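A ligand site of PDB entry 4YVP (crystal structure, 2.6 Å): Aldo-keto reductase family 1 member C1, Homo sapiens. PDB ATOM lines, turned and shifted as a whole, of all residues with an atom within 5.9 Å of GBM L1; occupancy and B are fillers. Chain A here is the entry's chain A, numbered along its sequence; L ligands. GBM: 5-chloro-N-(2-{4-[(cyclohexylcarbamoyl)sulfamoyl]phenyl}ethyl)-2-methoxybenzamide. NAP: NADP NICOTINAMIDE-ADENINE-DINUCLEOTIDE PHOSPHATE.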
ATOM      1  N   TYR A  24     -13.830   7.640  -8.442  1.00  0.00           N
ATOM      2  CA  TYR A  24     -13.450   7.687  -9.833  1.00  0.00           C
ATOM      3  C   TYR A  24     -14.052   6.504 -10.579  1.00  0.00           C
ATOM      4  O   TYR A  24     -14.022   5.375 -10.102  1.00  0.00           O
ATOM      5  CB  TYR A  24     -11.948   7.710 -10.068  1.00  0.00           C
ATOM      6  CG  TYR A  24     -11.645   7.774 -11.542  1.00  0.00           C
ATOM      7  CD1 TYR A  24     -11.931   8.918 -12.298  1.00  0.00           C
ATOM      8  CD2 TYR A  24     -11.136   6.669 -12.227  1.00  0.00           C
ATOM      9  CE1 TYR A  24     -11.664   8.987 -13.667  1.00  0.00           C
ATOM     10  CE2 TYR A  24     -10.866   6.723 -13.588  1.00  0.00           C
ATOM     11  CZ  TYR A  24     -11.127   7.885 -14.309  1.00  0.00           C
ATOM     12  OH  TYR A  24     -10.863   7.947 -15.667  1.00  0.00           O
ATOM     13  N   ALA A  52     -11.423  14.273  -6.452  1.00  0.00           N
ATOM     14  CA  ALA A  52     -10.426  15.213  -6.937  1.00  0.00           C
ATOM     15  C   ALA A  52     -11.068  16.102  -7.976  1.00  0.00           C
ATOM     16  O   ALA A  52     -12.124  15.771  -8.525  1.00  0.00           O
ATOM     17  CB  ALA A  52      -9.271  14.467  -7.565  1.00  0.00           C
ATOM     18  N   LEU A  54      -9.601  16.597 -10.925  1.00  0.00           N
ATOM     19  CA  LEU A  54      -9.367  15.715 -12.051  1.00  0.00           C
ATOM     20  C   LEU A  54     -10.520  14.736 -12.393  1.00  0.00           C
ATOM     21  O   LEU A  54     -10.790  14.484 -13.557  1.00  0.00           O
ATOM     22  CB  LEU A  54      -8.106  14.896 -11.816  1.00  0.00           C
ATOM     23  CG  LEU A  54      -7.623  14.049 -13.000  1.00  0.00           C
ATOM     24  CD1 LEU A  54      -7.081  14.912 -14.129  1.00  0.00           C
ATOM     25  CD2 LEU A  54      -6.556  13.079 -12.563  1.00  0.00           C
ATOM     26  N   TYR A  55     -11.196  14.192 -11.398  1.00  0.00           N
ATOM     27  CA  TYR A  55     -12.181  13.149 -11.657  1.00  0.00           C
ATOM     28  C   TYR A  55     -13.444  13.709 -12.320  1.00  0.00           C
ATOM     29  O   TYR A  55     -14.331  12.942 -12.715  1.00  0.00           O
ATOM     30  CB  TYR A  55     -12.537  12.381 -10.376  1.00  0.00           C
ATOM     31  CG  TYR A  55     -11.336  11.793  -9.642  1.00  0.00           C
ATOM     32  CD1 TYR A  55     -10.157  11.515 -10.301  1.00  0.00           C
ATOM     33  CD2 TYR A  55     -11.405  11.485  -8.294  1.00  0.00           C
ATOM     34  CE1 TYR A  55      -9.079  10.996  -9.637  1.00  0.00           C
ATOM     35  CE2 TYR A  55     -10.311  10.950  -7.627  1.00  0.00           C
ATOM     36  CZ  TYR A  55      -9.153  10.710  -8.318  1.00  0.00           C
ATOM     37  OH  TYR A  55      -8.017  10.198  -7.747  1.00  0.00           O
ATOM     38  N   ASN A  56     -13.534  15.039 -12.412  1.00  0.00           N
ATOM     39  CA  ASN A  56     -14.622  15.680 -13.095  1.00  0.00           C
ATOM     40  C   ASN A  56     -16.006  15.199 -12.596  1.00  0.00           C
ATOM     41  O   ASN A  56     -16.930  15.018 -13.394  1.00  0.00           O
ATOM     42  CB  ASN A  56     -14.442  15.456 -14.601  1.00  0.00           C
ATOM     43  CG  ASN A  56     -15.404  16.265 -15.430  1.00  0.00           C
ATOM     44  OD1 ASN A  56     -15.890  17.337 -15.024  1.00  0.00           O
ATOM     45  ND2 ASN A  56     -15.719  15.755 -16.615  1.00  0.00           N
ATOM     46  N   LYS A  84      -8.452  17.046  -4.305  1.00  0.00           N
ATOM     47  CA  LYS A  84      -7.031  17.136  -4.652  1.00  0.00           C
ATOM     48  C   LYS A  84      -6.706  18.264  -5.671  1.00  0.00           C
ATOM     49  O   LYS A  84      -7.388  18.480  -6.676  1.00  0.00           O
ATOM     50  CB  LYS A  84      -6.528  15.753  -5.122  1.00  0.00           C
ATOM     51  CG  LYS A  84      -6.948  14.538  -4.264  1.00  0.00           C
ATOM     52  CD  LYS A  84      -6.198  13.288  -4.740  1.00  0.00           C
ATOM     53  CE  LYS A  84      -6.769  11.997  -4.160  1.00  0.00           C
ATOM     54  NZ  LYS A  84      -8.029  11.543  -4.833  1.00  0.00           N
ATOM     55  N   TRP A  86      -4.990  19.594  -8.641  1.00  0.00           N
ATOM     56  CA  TRP A  86      -4.424  19.099  -9.883  1.00  0.00           C
ATOM     57  C   TRP A  86      -3.173  19.946 -10.283  1.00  0.00           C
ATOM     58  O   TRP A  86      -2.975  21.084  -9.826  1.00  0.00           O
ATOM     59  CB  TRP A  86      -5.502  18.984 -10.981  1.00  0.00           C
ATOM     60  CG  TRP A  86      -4.970  18.327 -12.229  1.00  0.00           C
ATOM     61  CD1 TRP A  86      -4.943  18.847 -13.486  1.00  0.00           C
ATOM     62  CD2 TRP A  86      -4.297  17.059 -12.317  1.00  0.00           C
ATOM     63  NE1 TRP A  86      -4.318  17.984 -14.351  1.00  0.00           N
ATOM     64  CE2 TRP A  86      -3.895  16.883 -13.656  1.00  0.00           C
ATOM     65  CE3 TRP A  86      -3.980  16.061 -11.377  1.00  0.00           C
ATOM     66  CZ2 TRP A  86      -3.206  15.749 -14.106  1.00  0.00           C
ATOM     67  CZ3 TRP A  86      -3.298  14.921 -11.824  1.00  0.00           C
ATOM     68  CH2 TRP A  86      -2.916  14.775 -13.175  1.00  0.00           C
ATOM     69  N   HIS A 117      -2.309  16.391  -5.463  1.00  0.00           N
ATOM     70  CA  HIS A 117      -2.638  15.205  -6.227  1.00  0.00           C
ATOM     71  C   HIS A 117      -1.419  14.486  -6.772  1.00  0.00           C
ATOM     72  O   HIS A 117      -1.278  13.278  -6.617  1.00  0.00           O
ATOM     73  CB  HIS A 117      -3.554  15.593  -7.397  1.00  0.00           C
ATOM     74  CG  HIS A 117      -4.337  14.457  -7.967  1.00  0.00           C
ATOM     75  ND1 HIS A 117      -5.527  14.644  -8.636  1.00  0.00           N
ATOM     76  CD2 HIS A 117      -4.139  13.115  -7.926  1.00  0.00           C
ATOM     77  CE1 HIS A 117      -6.022  13.479  -8.989  1.00  0.00           C
ATOM     78  NE2 HIS A 117      -5.199  12.533  -8.558  1.00  0.00           N
ATOM     79  N   PHE A 118      -0.542  15.216  -7.459  1.00  0.00           N
ATOM     80  CA  PHE A 118       0.653  14.623  -8.083  1.00  0.00           C
ATOM     81  C   PHE A 118       1.802  15.623  -8.070  1.00  0.00           C
ATOM     82  O   PHE A 118       1.554  16.825  -8.252  1.00  0.00           O
ATOM     83  CB  PHE A 118       0.323  14.209  -9.508  1.00  0.00           C
ATOM     84  CG  PHE A 118       1.265  13.184 -10.079  1.00  0.00           C
ATOM     85  CD1 PHE A 118       1.322  11.902  -9.548  1.00  0.00           C
ATOM     86  CD2 PHE A 118       2.086  13.487 -11.159  1.00  0.00           C
ATOM     87  CE1 PHE A 118       2.183  10.972 -10.052  1.00  0.00           C
ATOM     88  CE2 PHE A 118       2.963  12.541 -11.661  1.00  0.00           C
ATOM     89  CZ  PHE A 118       3.001  11.282 -11.119  1.00  0.00           C
ATOM     90  N   VAL A 128      -6.259  19.799 -19.073  1.00  0.00           N
ATOM     91  CA  VAL A 128      -5.949  18.928 -17.944  1.00  0.00           C
ATOM     92  C   VAL A 128      -4.469  18.490 -17.981  1.00  0.00           C
ATOM     93  O   VAL A 128      -3.735  18.719 -17.024  1.00  0.00           O
ATOM     94  CB  VAL A 128      -6.905  17.708 -17.942  1.00  0.00           C
ATOM     95  CG1 VAL A 128      -6.472  16.657 -16.917  1.00  0.00           C
ATOM     96  CG2 VAL A 128      -8.345  18.149 -17.690  1.00  0.00           C
ATOM     97  N   ILE A 129      -4.084  17.858 -19.093  1.00  0.00           N
ATOM     98  CA  ILE A 129      -2.717  17.431 -19.387  1.00  0.00           C
ATOM     99  C   ILE A 129      -2.305  18.071 -20.737  1.00  0.00           C
ATOM    100  O   ILE A 129      -2.435  17.437 -21.797  1.00  0.00           O
ATOM    101  CB  ILE A 129      -2.585  15.872 -19.465  1.00  0.00           C
ATOM    102  CG1 ILE A 129      -2.947  15.237 -18.126  1.00  0.00           C
ATOM    103  CG2 ILE A 129      -1.165  15.436 -19.795  1.00  0.00           C
ATOM    104  CD1 ILE A 129      -3.484  13.824 -18.245  1.00  0.00           C
ATOM    105  N   LYS A 131      -0.224  19.113 -23.833  1.00  0.00           N
ATOM    106  CA  LYS A 131       0.965  18.610 -24.547  1.00  0.00           C
ATOM    107  C   LYS A 131       1.170  19.451 -25.808  1.00  0.00           C
ATOM    108  O   LYS A 131       0.249  20.135 -26.257  1.00  0.00           O
ATOM    109  CB  LYS A 131       0.814  17.119 -24.952  1.00  0.00           C
ATOM    110  CG  LYS A 131       0.263  16.188 -23.868  1.00  0.00           C
ATOM    111  CD  LYS A 131       0.122  14.751 -24.373  1.00  0.00           C
ATOM    112  CE  LYS A 131      -1.002  13.966 -23.674  1.00  0.00           C
ATOM    113  NZ  LYS A 131      -2.360  14.328 -24.186  1.00  0.00           N
ATOM    114  N   ASN A 167       1.087  10.576  -4.028  1.00  0.00           N
ATOM    115  CA  ASN A 167       2.135  10.171  -5.001  1.00  0.00           C
ATOM    116  C   ASN A 167       3.486  10.843  -4.775  1.00  0.00           C
ATOM    117  O   ASN A 167       4.226  11.067  -5.701  1.00  0.00           O
ATOM    118  CB  ASN A 167       1.671  10.364  -6.473  1.00  0.00           C
ATOM    119  CG  ASN A 167       0.327   9.701  -6.769  1.00  0.00           C
ATOM    120  OD1 ASN A 167      -0.650  10.383  -7.070  1.00  0.00           O
ATOM    121  ND2 ASN A 167       0.267   8.389  -6.683  1.00  0.00           N
ATOM    122  N   TYR A 216      -4.615   3.631  -2.334  1.00  0.00           N
ATOM    123  CA  TYR A 216      -5.528   3.621  -3.491  1.00  0.00           C
ATOM    124  C   TYR A 216      -5.223   2.456  -4.438  1.00  0.00           C
ATOM    125  O   TYR A 216      -4.149   1.863  -4.375  1.00  0.00           O
ATOM    126  CB  TYR A 216      -5.554   4.966  -4.230  1.00  0.00           C
ATOM    127  CG  TYR A 216      -4.366   5.335  -5.101  1.00  0.00           C
ATOM    128  CD1 TYR A 216      -4.013   4.594  -6.238  1.00  0.00           C
ATOM    129  CD2 TYR A 216      -3.612   6.471  -4.826  1.00  0.00           C
ATOM    130  CE1 TYR A 216      -2.943   4.960  -7.043  1.00  0.00           C
ATOM    131  CE2 TYR A 216      -2.552   6.846  -5.636  1.00  0.00           C
ATOM    132  CZ  TYR A 216      -2.228   6.084  -6.751  1.00  0.00           C
ATOM    133  OH  TYR A 216      -1.192   6.454  -7.561  1.00  0.00           O
ATOM    134  N   SER A 217      -6.150   2.189  -5.352  1.00  0.00           N
ATOM    135  CA  SER A 217      -6.107   0.986  -6.170  1.00  0.00           C
ATOM    136  C   SER A 217      -5.865  -0.246  -5.267  1.00  0.00           C
ATOM    137  O   SER A 217      -5.119  -1.161  -5.617  1.00  0.00           O
ATOM    138  CB  SER A 217      -5.098   1.096  -7.329  1.00  0.00           C
ATOM    139  OG  SER A 217      -5.414   2.230  -8.148  1.00  0.00           O
ATOM    140  N   HIS A 222      -8.987   0.187 -11.332  1.00  0.00           N
ATOM    141  CA  HIS A 222      -9.926   0.200 -12.464  1.00  0.00           C
ATOM    142  C   HIS A 222      -9.461  -0.493 -13.750  1.00  0.00           C
ATOM    143  O   HIS A 222     -10.281  -0.813 -14.597  1.00  0.00           O
ATOM    144  CB  HIS A 222     -10.261   1.663 -12.808  1.00  0.00           C
ATOM    145  CG  HIS A 222      -9.070   2.588 -12.764  1.00  0.00           C
ATOM    146  ND1 HIS A 222      -7.933   2.402 -13.519  1.00  0.00           N
ATOM    147  CD2 HIS A 222      -8.846   3.705 -12.034  1.00  0.00           C
ATOM    148  CE1 HIS A 222      -7.065   3.354 -13.267  1.00  0.00           C
ATOM    149  NE2 HIS A 222      -7.596   4.153 -12.363  1.00  0.00           N
ATOM    150  N   GLU A 224      -8.276   0.758 -16.345  1.00  0.00           N
ATOM    151  CA  GLU A 224      -8.517   1.603 -17.475  1.00  0.00           C
ATOM    152  C   GLU A 224      -7.256   1.829 -18.291  1.00  0.00           C
ATOM    153  O   GLU A 224      -6.251   2.256 -17.744  1.00  0.00           O
ATOM    154  CB  GLU A 224      -9.057   2.960 -17.012  1.00  0.00           C
ATOM    155  CG  GLU A 224      -9.173   3.974 -18.144  1.00  0.00           C
ATOM    156  CD  GLU A 224      -9.736   5.306 -17.727  1.00  0.00           C
ATOM    157  OE1 GLU A 224     -10.283   5.956 -18.640  1.00  0.00           O
ATOM    158  OE2 GLU A 224      -9.622   5.709 -16.545  1.00  0.00           O
ATOM    159  N   TRP A 227      -3.951   3.939 -18.760  1.00  0.00           N
ATOM    160  CA  TRP A 227      -3.397   4.151 -17.454  1.00  0.00           C
ATOM    161  C   TRP A 227      -2.868   2.870 -16.867  1.00  0.00           C
ATOM    162  O   TRP A 227      -1.995   2.925 -16.031  1.00  0.00           O
ATOM    163  CB  TRP A 227      -4.452   4.771 -16.517  1.00  0.00           C
ATOM    164  CG  TRP A 227      -4.975   6.044 -17.108  1.00  0.00           C
ATOM    165  CD1 TRP A 227      -6.149   6.216 -17.775  1.00  0.00           C
ATOM    166  CD2 TRP A 227      -4.305   7.292 -17.140  1.00  0.00           C
ATOM    167  NE1 TRP A 227      -6.260   7.511 -18.191  1.00  0.00           N
ATOM    168  CE2 TRP A 227      -5.139   8.193 -17.823  1.00  0.00           C
ATOM    169  CE3 TRP A 227      -3.079   7.741 -16.640  1.00  0.00           C
ATOM    170  CZ2 TRP A 227      -4.800   9.519 -18.016  1.00  0.00           C
ATOM    171  CZ3 TRP A 227      -2.736   9.052 -16.824  1.00  0.00           C
ATOM    172  CH2 TRP A 227      -3.601   9.941 -17.505  1.00  0.00           C
ATOM    173  N   LEU A 306      -0.369   1.838 -11.584  1.00  0.00           N
ATOM    174  CA  LEU A 306      -0.367   3.227 -12.035  1.00  0.00           C
ATOM    175  C   LEU A 306       1.022   3.801 -12.066  1.00  0.00           C
ATOM    176  O   LEU A 306       1.428   4.515 -11.141  1.00  0.00           O
ATOM    177  CB  LEU A 306      -1.291   4.082 -11.175  1.00  0.00           C
ATOM    178  CG  LEU A 306      -2.743   3.937 -11.636  1.00  0.00           C
ATOM    179  CD1 LEU A 306      -3.644   4.498 -10.566  1.00  0.00           C
ATOM    180  CD2 LEU A 306      -3.014   4.629 -12.963  1.00  0.00           C
ATOM    181  N   LEU A 308       2.044   5.877 -14.458  1.00  0.00           N
ATOM    182  CA  LEU A 308       1.955   7.277 -14.854  1.00  0.00           C
ATOM    183  C   LEU A 308       3.160   7.748 -15.681  1.00  0.00           C
ATOM    184  O   LEU A 308       3.642   8.872 -15.502  1.00  0.00           O
ATOM    185  CB  LEU A 308       1.706   8.142 -13.623  1.00  0.00           C
ATOM    186  CG  LEU A 308       0.465   7.682 -12.857  1.00  0.00           C
ATOM    187  CD1 LEU A 308       0.392   8.359 -11.500  1.00  0.00           C
ATOM    188  CD2 LEU A 308      -0.775   7.971 -13.694  1.00  0.00           C
ATOM    189  N   PHE A 311       4.140  11.132 -17.215  1.00  0.00           N
ATOM    190  CA  PHE A 311       4.760  12.139 -16.379  1.00  0.00           C
ATOM    191  C   PHE A 311       6.248  11.992 -16.111  1.00  0.00           C
ATOM    192  O   PHE A 311       6.833  12.877 -15.489  1.00  0.00           O
ATOM    193  CB  PHE A 311       4.009  12.233 -15.059  1.00  0.00           C
ATOM    194  CG  PHE A 311       2.644  12.807 -15.209  1.00  0.00           C
ATOM    195  CD1 PHE A 311       2.504  14.158 -15.408  1.00  0.00           C
ATOM    196  CD2 PHE A 311       1.518  11.994 -15.175  1.00  0.00           C
ATOM    197  CE1 PHE A 311       1.245  14.725 -15.564  1.00  0.00           C
ATOM    198  CE2 PHE A 311       0.246  12.547 -15.325  1.00  0.00           C
ATOM    199  CZ  PHE A 311       0.112  13.912 -15.515  1.00  0.00           C
HETATM  200  O3  GBM L   1      -5.947  10.292  -9.393  1.00  0.00           O
HETATM  201  O4  GBM L   1      -6.257   6.408 -11.140  1.00  0.00           O
HETATM  202  O5  GBM L   1      -8.655   6.623 -10.557  1.00  0.00           O
HETATM  203  O6  GBM L   1      -9.792  12.990 -16.523  1.00  0.00           O
HETATM  204 CL1  GBM L   1     -12.389  16.272 -19.514  1.00  0.00          CL
HETATM  205  S2  GBM L   1      -7.429   7.218 -10.986  1.00  0.00           S
HETATM  206  O7  GBM L   1      -7.255  13.462 -19.774  1.00  0.00           O
HETATM  207  N8  GBM L   1      -5.154   8.919 -11.060  1.00  0.00           N
HETATM  208  N9  GBM L   1      -7.108   8.406  -9.909  1.00  0.00           N
HETATM  209  N10 GBM L   1      -8.009  12.128 -17.585  1.00  0.00           N
HETATM  210  C11 GBM L   1      -3.956   9.624 -11.511  1.00  0.00           C
HETATM  211  C12 GBM L   1      -3.096  10.229 -10.408  1.00  0.00           C
HETATM  212  C13 GBM L   1      -4.267  10.641 -12.574  1.00  0.00           C
HETATM  213  C14 GBM L   1      -2.329  11.460 -10.896  1.00  0.00           C
HETATM  214  C15 GBM L   1      -2.990  11.068 -13.293  1.00  0.00           C
HETATM  215  C16 GBM L   1      -1.840  11.311 -12.319  1.00  0.00           C
HETATM  216  C17 GBM L   1      -6.018   9.268 -10.055  1.00  0.00           C
HETATM  217  C18 GBM L   1      -7.730   8.020 -12.523  1.00  0.00           C
HETATM  218  C19 GBM L   1      -7.958   9.429 -14.911  1.00  0.00           C
HETATM  219  C20 GBM L   1      -8.217  10.106 -16.244  1.00  0.00           C
HETATM  220  C21 GBM L   1      -8.477   9.179 -12.564  1.00  0.00           C
HETATM  221  C22 GBM L   1      -7.114   7.539 -13.675  1.00  0.00           C
HETATM  222  C23 GBM L   1      -8.565   9.888 -13.753  1.00  0.00           C
HETATM  223  C24 GBM L   1      -7.228   8.249 -14.853  1.00  0.00           C
HETATM  224  C25 GBM L   1      -7.513  11.393 -16.423  1.00  0.00           C
HETATM  225  C26 GBM L   1      -9.049  12.968 -17.502  1.00  0.00           C
HETATM  226  C27 GBM L   1      -9.279  13.912 -18.652  1.00  0.00           C
HETATM  227  C28 GBM L   1      -8.394  14.223 -19.695  1.00  0.00           C
HETATM  228  C29 GBM L   1     -10.515  14.568 -18.602  1.00  0.00           C
HETATM  229  C30 GBM L   1      -8.730  15.194 -20.639  1.00  0.00           C
HETATM  230  C31 GBM L   1     -10.827  15.509 -19.559  1.00  0.00           C
HETATM  231  C32 GBM L   1      -9.958  15.834 -20.571  1.00  0.00           C
HETATM  232  C33 GBM L   1      -6.146  13.931 -20.556  1.00  0.00           C
HETATM  233  PA  NAP L   2      -9.896  -0.024  -6.776  1.00  0.00           P
HETATM  234  O1A NAP L   2     -10.952   0.716  -5.985  1.00  0.00           O
HETATM  235  O2A NAP L   2      -8.817  -0.806  -6.099  1.00  0.00           O
HETATM  236  O5B NAP L   2     -10.519  -1.184  -7.699  1.00  0.00           O
HETATM  237  C5B NAP L   2     -11.892  -1.083  -7.902  1.00  0.00           C
HETATM  238  C4B NAP L   2     -12.346  -2.058  -8.935  1.00  0.00           C
HETATM  239  O4B NAP L   2     -12.733  -3.226  -8.211  1.00  0.00           O
HETATM  240  C3B NAP L   2     -13.591  -1.553  -9.655  1.00  0.00           C
HETATM  241  O3B NAP L   2     -13.588  -2.058 -10.977  1.00  0.00           O
HETATM  242  C2B NAP L   2     -14.735  -2.148  -8.866  1.00  0.00           C
HETATM  243  O2B NAP L   2     -15.809  -2.473  -9.705  1.00  0.00           O
HETATM  244  C1B NAP L   2     -14.144  -3.438  -8.330  1.00  0.00           C
HETATM  245  N9A NAP L   2     -14.674  -3.856  -7.019  1.00  0.00           N
HETATM  246  C8A NAP L   2     -15.044  -3.066  -5.991  1.00  0.00           C
HETATM  247  N7A NAP L   2     -15.503  -3.796  -4.947  1.00  0.00           N
HETATM  248  C5A NAP L   2     -15.407  -5.084  -5.330  1.00  0.00           C
HETATM  249  C6A NAP L   2     -15.710  -6.361  -4.697  1.00  0.00           C
HETATM  250  N6A NAP L   2     -16.205  -6.373  -3.471  1.00  0.00           N
HETATM  251  N1A NAP L   2     -15.502  -7.479  -5.408  1.00  0.00           N
HETATM  252  C2A NAP L   2     -15.010  -7.451  -6.675  1.00  0.00           C
HETATM  253  N3A NAP L   2     -14.702  -6.311  -7.299  1.00  0.00           N
HETATM  254  C4A NAP L   2     -14.864  -5.127  -6.682  1.00  0.00           C
HETATM  255  O3  NAP L   2      -9.194   0.906  -7.887  1.00  0.00           O
HETATM  256  PN  NAP L   2      -9.277   2.492  -8.206  1.00  0.00           P
HETATM  257  O1N NAP L   2     -10.677   2.797  -8.636  1.00  0.00           O
HETATM  258  O2N NAP L   2      -8.127   2.704  -9.158  1.00  0.00           O
HETATM  259  O5D NAP L   2      -9.025   3.267  -6.817  1.00  0.00           O
HETATM  260  C5D NAP L   2     -10.118   3.733  -6.029  1.00  0.00           C
HETATM  261  C4D NAP L   2     -10.017   5.209  -5.712  1.00  0.00           C
HETATM  262  O4D NAP L   2      -8.691   5.546  -5.388  1.00  0.00           O
HETATM  263  C3D NAP L   2     -10.389   6.114  -6.876  1.00  0.00           C
HETATM  264  O3D NAP L   2     -11.797   6.308  -7.045  1.00  0.00           O
HETATM  265  C2D NAP L   2      -9.735   7.385  -6.446  1.00  0.00           C
HETATM  266  O2D NAP L   2     -10.614   7.963  -5.462  1.00  0.00           O
HETATM  267  C1D NAP L   2      -8.480   6.896  -5.774  1.00  0.00           C
HETATM  268  N1N NAP L   2      -7.271   6.949  -6.600  1.00  0.00           N
HETATM  269  C2N NAP L   2      -6.382   7.935  -6.323  1.00  0.00           C
HETATM  270  C3N NAP L   2      -5.194   8.090  -7.021  1.00  0.00           C
HETATM  271  C7N NAP L   2      -4.253   9.210  -6.647  1.00  0.00           C
HETATM  272  O7N NAP L   2      -4.412   9.821  -5.598  1.00  0.00           O
HETATM  273  N7N NAP L   2      -3.196   9.482  -7.386  1.00  0.00           N
HETATM  274  C4N NAP L   2      -4.907   7.134  -8.011  1.00  0.00           C
HETATM  275  C5N NAP L   2      -5.823   6.120  -8.244  1.00  0.00           C
HETATM  276  C6N NAP L   2      -7.012   6.021  -7.520  1.00  0.00           C
HETATM  277  P2B NAP L   2     -17.307  -1.999  -9.479  1.00  0.00           P
HETATM  278  O1X NAP L   2     -17.300  -0.487  -9.349  1.00  0.00           O
HETATM  279  O2X NAP L   2     -17.824  -2.554 -10.772  1.00  0.00           O
HETATM  280  O3X NAP L   2     -17.811  -2.760  -8.294  1.00  0.00           O
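An oxygen (O3) of GBM L1 sits at hydrogen-bond distance from a ring nitrogen (NE2) of His 117 (2.5 Å). OH of Tyr 55 is in hydrogen-bond range of O3 of GBM L1. An oxygen (O4) of GBM L1 is in hydrogen-bond range of a ring nitrogen (NE2) of His 222, 2.9 Å away. An oxygen (O2N) of NAP L2 sits close to the backbone NH of His 222, 3.4 Å away. An oxygen (O3D) of NAP L2 lies within hydrogen-bond range of the backbone NH of Tyr 24 (2.8 Å). The side-chain amide oxygen (OD1) of Asn 167 is in hydrogen-bond range of a nitrogen (N7N) of NAP L2 (2.7 Å). The backbone NH (N) of Ser 217 is in hydrogen-bond range of an oxygen (O5D) of NAP L2, 3.4 Å away. O2N of NAP L2 lies within hydrogen-bond range of OG of Ser 217.
OD1 of Asn 167 sits close to O of His 117, at 3.0 Å. The side-chain hydroxyl (OH) of Tyr 55 is in hydrogen-bond range of the side-chain amino group (NZ) of Lys 84, at 3.2 Å. A ring nitrogen (ND1) of His 222 lies close to the backbone NH (N) of Glu 224, at 3.3 Å. OH of Tyr 24 sits at hydrogen-bond distance from OE2 of Glu 224. The indole nitrogen of Trp 86 sits at hydrogen-bond distance from the backbone carbonyl oxygen of Val 128.
O6 of GBM L1 sits close to O of Leu 54 (3.5 Å). Residues that only touch GBM L1: Tyr 24, Leu 306, Ile 129, Trp 227, Trp 86, Leu 308, Phe 311, Glu 224 and Phe 118. Hydrophobic or aromatic side chains within 4 Å of GBM L1: Tyr 24, Leu 54, Tyr 55, Trp 86, His 117, Phe 118, Ile 129, His 222, Trp 227, Leu 306, Leu 308 and Phe 311.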
